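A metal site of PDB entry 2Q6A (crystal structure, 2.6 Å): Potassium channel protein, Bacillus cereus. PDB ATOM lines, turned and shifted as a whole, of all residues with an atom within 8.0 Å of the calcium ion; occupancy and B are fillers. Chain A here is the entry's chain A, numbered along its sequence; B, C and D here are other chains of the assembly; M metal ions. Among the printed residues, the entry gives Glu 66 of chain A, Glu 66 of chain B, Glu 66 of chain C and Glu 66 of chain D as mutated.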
ATOM      1  N   VAL A  59      11.976 -20.565  -5.006  1.00  0.00           N
ATOM      2  CA  VAL A  59      13.011 -20.684  -6.027  1.00  0.00           C
ATOM      3  C   VAL A  59      12.614 -20.072  -7.362  1.00  0.00           C
ATOM      4  O   VAL A  59      13.477 -19.707  -8.171  1.00  0.00           O
ATOM      5  CB  VAL A  59      13.424 -22.155  -6.286  1.00  0.00           C
ATOM      6  CG1 VAL A  59      13.692 -22.878  -4.971  1.00  0.00           C
ATOM      7  CG2 VAL A  59      12.385 -22.840  -7.149  1.00  0.00           C
ATOM      8  N   THR A  62      12.774 -16.119  -7.166  1.00  0.00           N
ATOM      9  CA  THR A  62      14.120 -15.617  -6.976  1.00  0.00           C
ATOM     10  C   THR A  62      15.055 -15.948  -8.137  1.00  0.00           C
ATOM     11  O   THR A  62      16.244 -15.666  -8.086  1.00  0.00           O
ATOM     12  CB  THR A  62      14.746 -16.134  -5.660  1.00  0.00           C
ATOM     13  OG1 THR A  62      14.795 -17.563  -5.666  1.00  0.00           O
ATOM     14  CG2 THR A  62      13.909 -15.685  -4.474  1.00  0.00           C
ATOM     15  N   THR A  63      14.475 -16.530  -9.196  1.00  0.00           N
ATOM     16  CA  THR A  63      15.183 -16.945 -10.405  1.00  0.00           C
ATOM     17  C   THR A  63      16.171 -18.091 -10.204  1.00  0.00           C
ATOM     18  O   THR A  63      16.889 -18.453 -11.132  1.00  0.00           O
ATOM     19  CB  THR A  63      15.955 -15.786 -11.097  1.00  0.00           C
ATOM     20  OG1 THR A  63      17.197 -15.567 -10.409  1.00  0.00           O
ATOM     21  CG2 THR A  63      15.118 -14.520 -11.116  1.00  0.00           C
ATOM     22  N   VAL A  64      16.214 -18.667  -9.008  1.00  0.00           N
ATOM     23  CA  VAL A  64      17.114 -19.797  -8.787  1.00  0.00           C
ATOM     24  C   VAL A  64      16.624 -20.901  -9.728  1.00  0.00           C
ATOM     25  O   VAL A  64      17.392 -21.430 -10.544  1.00  0.00           O
ATOM     26  CB  VAL A  64      17.069 -20.308  -7.308  1.00  0.00           C
ATOM     27  CG1 VAL A  64      17.926 -21.560  -7.159  1.00  0.00           C
ATOM     28  CG2 VAL A  64      17.594 -19.230  -6.378  1.00  0.00           C
ATOM     29  N   GLY A  65      15.326 -21.205  -9.625  1.00  0.00           N
ATOM     30  CA  GLY A  65      14.711 -22.215 -10.461  1.00  0.00           C
ATOM     31  C   GLY A  65      14.619 -23.588  -9.825  1.00  0.00           C
ATOM     32  O   GLY A  65      15.467 -23.951  -9.026  1.00  0.00           O
ATOM     33  N   GLU A  66      13.588 -24.353 -10.184  1.00  0.00           N
ATOM     34  CA  GLU A  66      13.395 -25.694  -9.652  1.00  0.00           C
ATOM     35  C   GLU A  66      13.863 -26.716 -10.700  1.00  0.00           C
ATOM     36  O   GLU A  66      13.475 -26.658 -11.867  1.00  0.00           O
ATOM     37  CB  GLU A  66      11.919 -25.906  -9.297  1.00  0.00           C
ATOM     38  CG  GLU A  66      11.717 -26.755  -8.058  1.00  0.00           C
ATOM     39  CD  GLU A  66      12.267 -28.151  -8.220  1.00  0.00           C
ATOM     40  OE1 GLU A  66      11.850 -28.834  -9.165  1.00  0.00           O
ATOM     41  OE2 GLU A  66      13.104 -28.578  -7.400  1.00  0.00           O
ATOM     42  N   VAL B  59      24.532 -20.895 -20.073  1.00  0.00           N
ATOM     43  CA  VAL B  59      23.470 -20.871 -19.078  1.00  0.00           C
ATOM     44  C   VAL B  59      23.990 -20.964 -17.652  1.00  0.00           C
ATOM     45  O   VAL B  59      23.314 -20.543 -16.704  1.00  0.00           O
ATOM     46  CB  VAL B  59      22.440 -22.010 -19.271  1.00  0.00           C
ATOM     47  CG1 VAL B  59      21.984 -22.072 -20.724  1.00  0.00           C
ATOM     48  CG2 VAL B  59      23.000 -23.316 -18.769  1.00  0.00           C
ATOM     49  N   THR B  62      25.593 -17.516 -16.542  1.00  0.00           N
ATOM     50  CA  THR B  62      24.625 -16.447 -16.445  1.00  0.00           C
ATOM     51  C   THR B  62      23.553 -16.692 -15.386  1.00  0.00           C
ATOM     52  O   THR B  62      22.611 -15.916 -15.259  1.00  0.00           O
ATOM     53  CB  THR B  62      23.935 -16.177 -17.814  1.00  0.00           C
ATOM     54  OG1 THR B  62      23.270 -17.358 -18.260  1.00  0.00           O
ATOM     55  CG2 THR B  62      24.977 -15.785 -18.842  1.00  0.00           C
ATOM     56  N   THR B  63      23.732 -17.775 -14.630  1.00  0.00           N
ATOM     57  CA  THR B  63      22.827 -18.207 -13.561  1.00  0.00           C
ATOM     58  C   THR B  63      21.455 -18.671 -14.046  1.00  0.00           C
ATOM     59  O   THR B  63      20.573 -18.960 -13.229  1.00  0.00           O
ATOM     60  CB  THR B  63      22.585 -17.120 -12.482  1.00  0.00           C
ATOM     61  OG1 THR B  63      21.625 -16.172 -12.954  1.00  0.00           O
ATOM     62  CG2 THR B  63      23.891 -16.433 -12.109  1.00  0.00           C
ATOM     63  N   VAL B  64      21.253 -18.745 -15.366  1.00  0.00           N
ATOM     64  CA  VAL B  64      19.970 -19.226 -15.871  1.00  0.00           C
ATOM     65  C   VAL B  64      19.853 -20.672 -15.380  1.00  0.00           C
ATOM     66  O   VAL B  64      18.869 -21.044 -14.723  1.00  0.00           O
ATOM     67  CB  VAL B  64      19.896 -19.196 -17.422  1.00  0.00           C
ATOM     68  CG1 VAL B  64      18.600 -19.824 -17.907  1.00  0.00           C
ATOM     69  CG2 VAL B  64      19.974 -17.760 -17.921  1.00  0.00           C
ATOM     70  N   GLY B  65      20.890 -21.461 -15.677  1.00  0.00           N
ATOM     71  CA  GLY B  65      20.938 -22.851 -15.254  1.00  0.00           C
ATOM     72  C   GLY B  65      20.469 -23.837 -16.307  1.00  0.00           C
ATOM     73  O   GLY B  65      19.612 -23.511 -17.112  1.00  0.00           O
ATOM     74  N   GLU B  66      21.029 -25.046 -16.297  1.00  0.00           N
ATOM     75  CA  GLU B  66      20.653 -26.080 -17.257  1.00  0.00           C
ATOM     76  C   GLU B  66      19.709 -27.074 -16.555  1.00  0.00           C
ATOM     77  O   GLU B  66      19.992 -27.574 -15.467  1.00  0.00           O
ATOM     78  CB  GLU B  66      21.909 -26.789 -17.775  1.00  0.00           C
ATOM     79  CG  GLU B  66      21.818 -27.189 -19.225  1.00  0.00           C
ATOM     80  CD  GLU B  66      20.698 -28.169 -19.491  1.00  0.00           C
ATOM     81  OE1 GLU B  66      20.704 -29.233 -18.845  1.00  0.00           O
ATOM     82  OE2 GLU B  66      19.825 -27.895 -20.338  1.00  0.00           O
ATOM     83  N   VAL C  59      25.439 -23.535  -6.519  1.00  0.00           N
ATOM     84  CA  VAL C  59      24.450 -23.233  -7.543  1.00  0.00           C
ATOM     85  C   VAL C  59      23.152 -22.675  -6.948  1.00  0.00           C
ATOM     86  O   VAL C  59      22.400 -21.968  -7.636  1.00  0.00           O
ATOM     87  CB  VAL C  59      24.115 -24.457  -8.428  1.00  0.00           C
ATOM     88  CG1 VAL C  59      25.414 -25.030  -9.062  1.00  0.00           C
ATOM     89  CG2 VAL C  59      23.373 -25.502  -7.594  1.00  0.00           C
ATOM     90  N   THR C  62      23.739 -18.904  -5.468  1.00  0.00           N
ATOM     91  CA  THR C  62      23.917 -17.976  -6.595  1.00  0.00           C
ATOM     92  C   THR C  62      22.757 -17.908  -7.598  1.00  0.00           C
ATOM     93  O   THR C  62      22.886 -17.275  -8.640  1.00  0.00           O
ATOM     94  CB  THR C  62      25.189 -18.324  -7.401  1.00  0.00           C
ATOM     95  OG1 THR C  62      25.082 -19.672  -7.892  1.00  0.00           O
ATOM     96  CG2 THR C  62      26.434 -18.199  -6.539  1.00  0.00           C
ATOM     97  N   THR C  63      21.646 -18.555  -7.279  1.00  0.00           N
ATOM     98  CA  THR C  63      20.462 -18.580  -8.140  1.00  0.00           C
ATOM     99  C   THR C  63      20.663 -19.235  -9.486  1.00  0.00           C
ATOM    100  O   THR C  63      19.807 -19.083 -10.374  1.00  0.00           O
ATOM    101  CB  THR C  63      19.903 -17.185  -8.437  1.00  0.00           C
ATOM    102  OG1 THR C  63      20.720 -16.559  -9.423  1.00  0.00           O
ATOM    103  CG2 THR C  63      19.875 -16.328  -7.167  1.00  0.00           C
ATOM    104  N   VAL C  64      21.780 -19.938  -9.669  1.00  0.00           N
ATOM    105  CA  VAL C  64      21.999 -20.631 -10.943  1.00  0.00           C
ATOM    106  C   VAL C  64      20.997 -21.780 -11.005  1.00  0.00           C
ATOM    107  O   VAL C  64      20.257 -21.933 -11.974  1.00  0.00           O
ATOM    108  CB  VAL C  64      23.429 -21.192 -11.055  1.00  0.00           C
ATOM    109  CG1 VAL C  64      23.553 -22.069 -12.283  1.00  0.00           C
ATOM    110  CG2 VAL C  64      24.425 -20.054 -11.164  1.00  0.00           C
ATOM    111  N   GLY C  65      20.972 -22.568  -9.929  1.00  0.00           N
ATOM    112  CA  GLY C  65      20.053 -23.692  -9.828  1.00  0.00           C
ATOM    113  C   GLY C  65      20.669 -25.032 -10.218  1.00  0.00           C
ATOM    114  O   GLY C  65      21.580 -25.084 -11.030  1.00  0.00           O
ATOM    115  N   GLU C  66      20.170 -26.111  -9.635  1.00  0.00           N
ATOM    116  CA  GLU C  66      20.671 -27.449  -9.940  1.00  0.00           C
ATOM    117  C   GLU C  66      19.594 -28.138 -10.787  1.00  0.00           C
ATOM    118  O   GLU C  66      18.426 -28.144 -10.419  1.00  0.00           O
ATOM    119  CB  GLU C  66      20.916 -28.235  -8.655  1.00  0.00           C
ATOM    120  CG  GLU C  66      22.123 -29.168  -8.717  1.00  0.00           C
ATOM    121  CD  GLU C  66      22.014 -30.188  -9.826  1.00  0.00           C
ATOM    122  OE1 GLU C  66      21.010 -30.923  -9.860  1.00  0.00           O
ATOM    123  OE2 GLU C  66      22.934 -30.260 -10.659  1.00  0.00           O
ATOM    124  N   VAL D  59      11.055 -17.983 -18.571  1.00  0.00           N
ATOM    125  CA  VAL D  59      11.994 -18.496 -17.583  1.00  0.00           C
ATOM    126  C   VAL D  59      13.447 -18.402 -18.064  1.00  0.00           C
ATOM    127  O   VAL D  59      14.377 -18.362 -17.244  1.00  0.00           O
ATOM    128  CB  VAL D  59      11.686 -19.954 -17.181  1.00  0.00           C
ATOM    129  CG1 VAL D  59      10.226 -20.074 -16.660  1.00  0.00           C
ATOM    130  CG2 VAL D  59      11.961 -20.886 -18.355  1.00  0.00           C
ATOM    131  N   THR D  62      14.686 -14.503 -18.190  1.00  0.00           N
ATOM    132  CA  THR D  62      14.846 -14.012 -16.813  1.00  0.00           C
ATOM    133  C   THR D  62      15.833 -14.787 -15.943  1.00  0.00           C
ATOM    134  O   THR D  62      15.917 -14.540 -14.737  1.00  0.00           O
ATOM    135  CB  THR D  62      13.491 -14.009 -16.067  1.00  0.00           C
ATOM    136  OG1 THR D  62      12.955 -15.343 -16.059  1.00  0.00           O
ATOM    137  CG2 THR D  62      12.498 -13.080 -16.744  1.00  0.00           C
ATOM    138  N   THR D  63      16.573 -15.715 -16.532  1.00  0.00           N
ATOM    139  CA  THR D  63      17.553 -16.531 -15.828  1.00  0.00           C
ATOM    140  C   THR D  63      16.986 -17.431 -14.747  1.00  0.00           C
ATOM    141  O   THR D  63      17.738 -17.963 -13.931  1.00  0.00           O
ATOM    142  CB  THR D  63      18.641 -15.702 -15.139  1.00  0.00           C
ATOM    143  OG1 THR D  63      18.111 -15.142 -13.934  1.00  0.00           O
ATOM    144  CG2 THR D  63      19.143 -14.586 -16.051  1.00  0.00           C
ATOM    145  N   VAL D  64      15.664 -17.591 -14.717  1.00  0.00           N
ATOM    146  CA  VAL D  64      15.066 -18.490 -13.723  1.00  0.00           C
ATOM    147  C   VAL D  64      15.452 -19.909 -14.124  1.00  0.00           C
ATOM    148  O   VAL D  64      15.977 -20.678 -13.308  1.00  0.00           O
ATOM    149  CB  VAL D  64      13.531 -18.370 -13.689  1.00  0.00           C
ATOM    150  CG1 VAL D  64      12.941 -19.450 -12.807  1.00  0.00           C
ATOM    151  CG2 VAL D  64      13.128 -17.016 -13.141  1.00  0.00           C
ATOM    152  N   GLY D  65      15.225 -20.236 -15.392  1.00  0.00           N
ATOM    153  CA  GLY D  65      15.555 -21.546 -15.918  1.00  0.00           C
ATOM    154  C   GLY D  65      14.386 -22.527 -15.938  1.00  0.00           C
ATOM    155  O   GLY D  65      13.485 -22.436 -15.118  1.00  0.00           O
ATOM    156  N   GLU D  66      14.402 -23.458 -16.884  1.00  0.00           N
ATOM    157  CA  GLU D  66      13.348 -24.462 -16.984  1.00  0.00           C
ATOM    158  C   GLU D  66      13.942 -25.784 -16.501  1.00  0.00           C
ATOM    159  O   GLU D  66      15.015 -26.181 -16.940  1.00  0.00           O
ATOM    160  CB  GLU D  66      12.880 -24.595 -18.440  1.00  0.00           C
ATOM    161  CG  GLU D  66      11.386 -24.869 -18.591  1.00  0.00           C
ATOM    162  CD  GLU D  66      10.956 -26.134 -17.876  1.00  0.00           C
ATOM    163  OE1 GLU D  66      11.530 -27.201 -18.160  1.00  0.00           O
ATOM    164  OE2 GLU D  66      10.036 -26.062 -17.043  1.00  0.00           O
HETATM  165 CA    CA M   1      18.382 -20.202 -12.453  1.00  0.00          CA
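The calcium ion is bound by O of Val 64 of chain B (2.5 Å), O of Val 64 of chain A (2.5 Å), O of Val 64 of chain C (2.6 Å), O of Val 64 of chain D (2.6 Å), O of Thr 63 of chain B (2.6 Å), O of Thr 63 of chain A (2.7 Å), O of Thr 63 of chain C (2.8 Å) and O of Thr 63 of chain D (2.8 Å).
Eight residues have an atom within 4 Å of the calcium ion: Thr 63 of chain A, Val 64 of chain A, Thr 63 of chain B, Val 64 of chain B, Thr 63 of chain C, Val 64 of chain C, Thr 63 of chain D and Val 64 of chain D.
The nearest printed residue that does not touch the calcium ion is Gly 65 of chain B (4.3 Å).
The backbone NH of Val 64 of chain D lies within hydrogen-bond range of the backbone carbonyl oxygen of Val 59 of chain D, 2.9 Å away.
The backbone NH (N) of Val 64 of chain A is in hydrogen-bond range of the backbone carbonyl oxygen (O) of Val 59 of chain A (3.0 Å).
The backbone NH of Val 64 of chain C sits at hydrogen-bond distance from the backbone carbonyl oxygen of Val 59 of chain C, 2.9 Å away.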
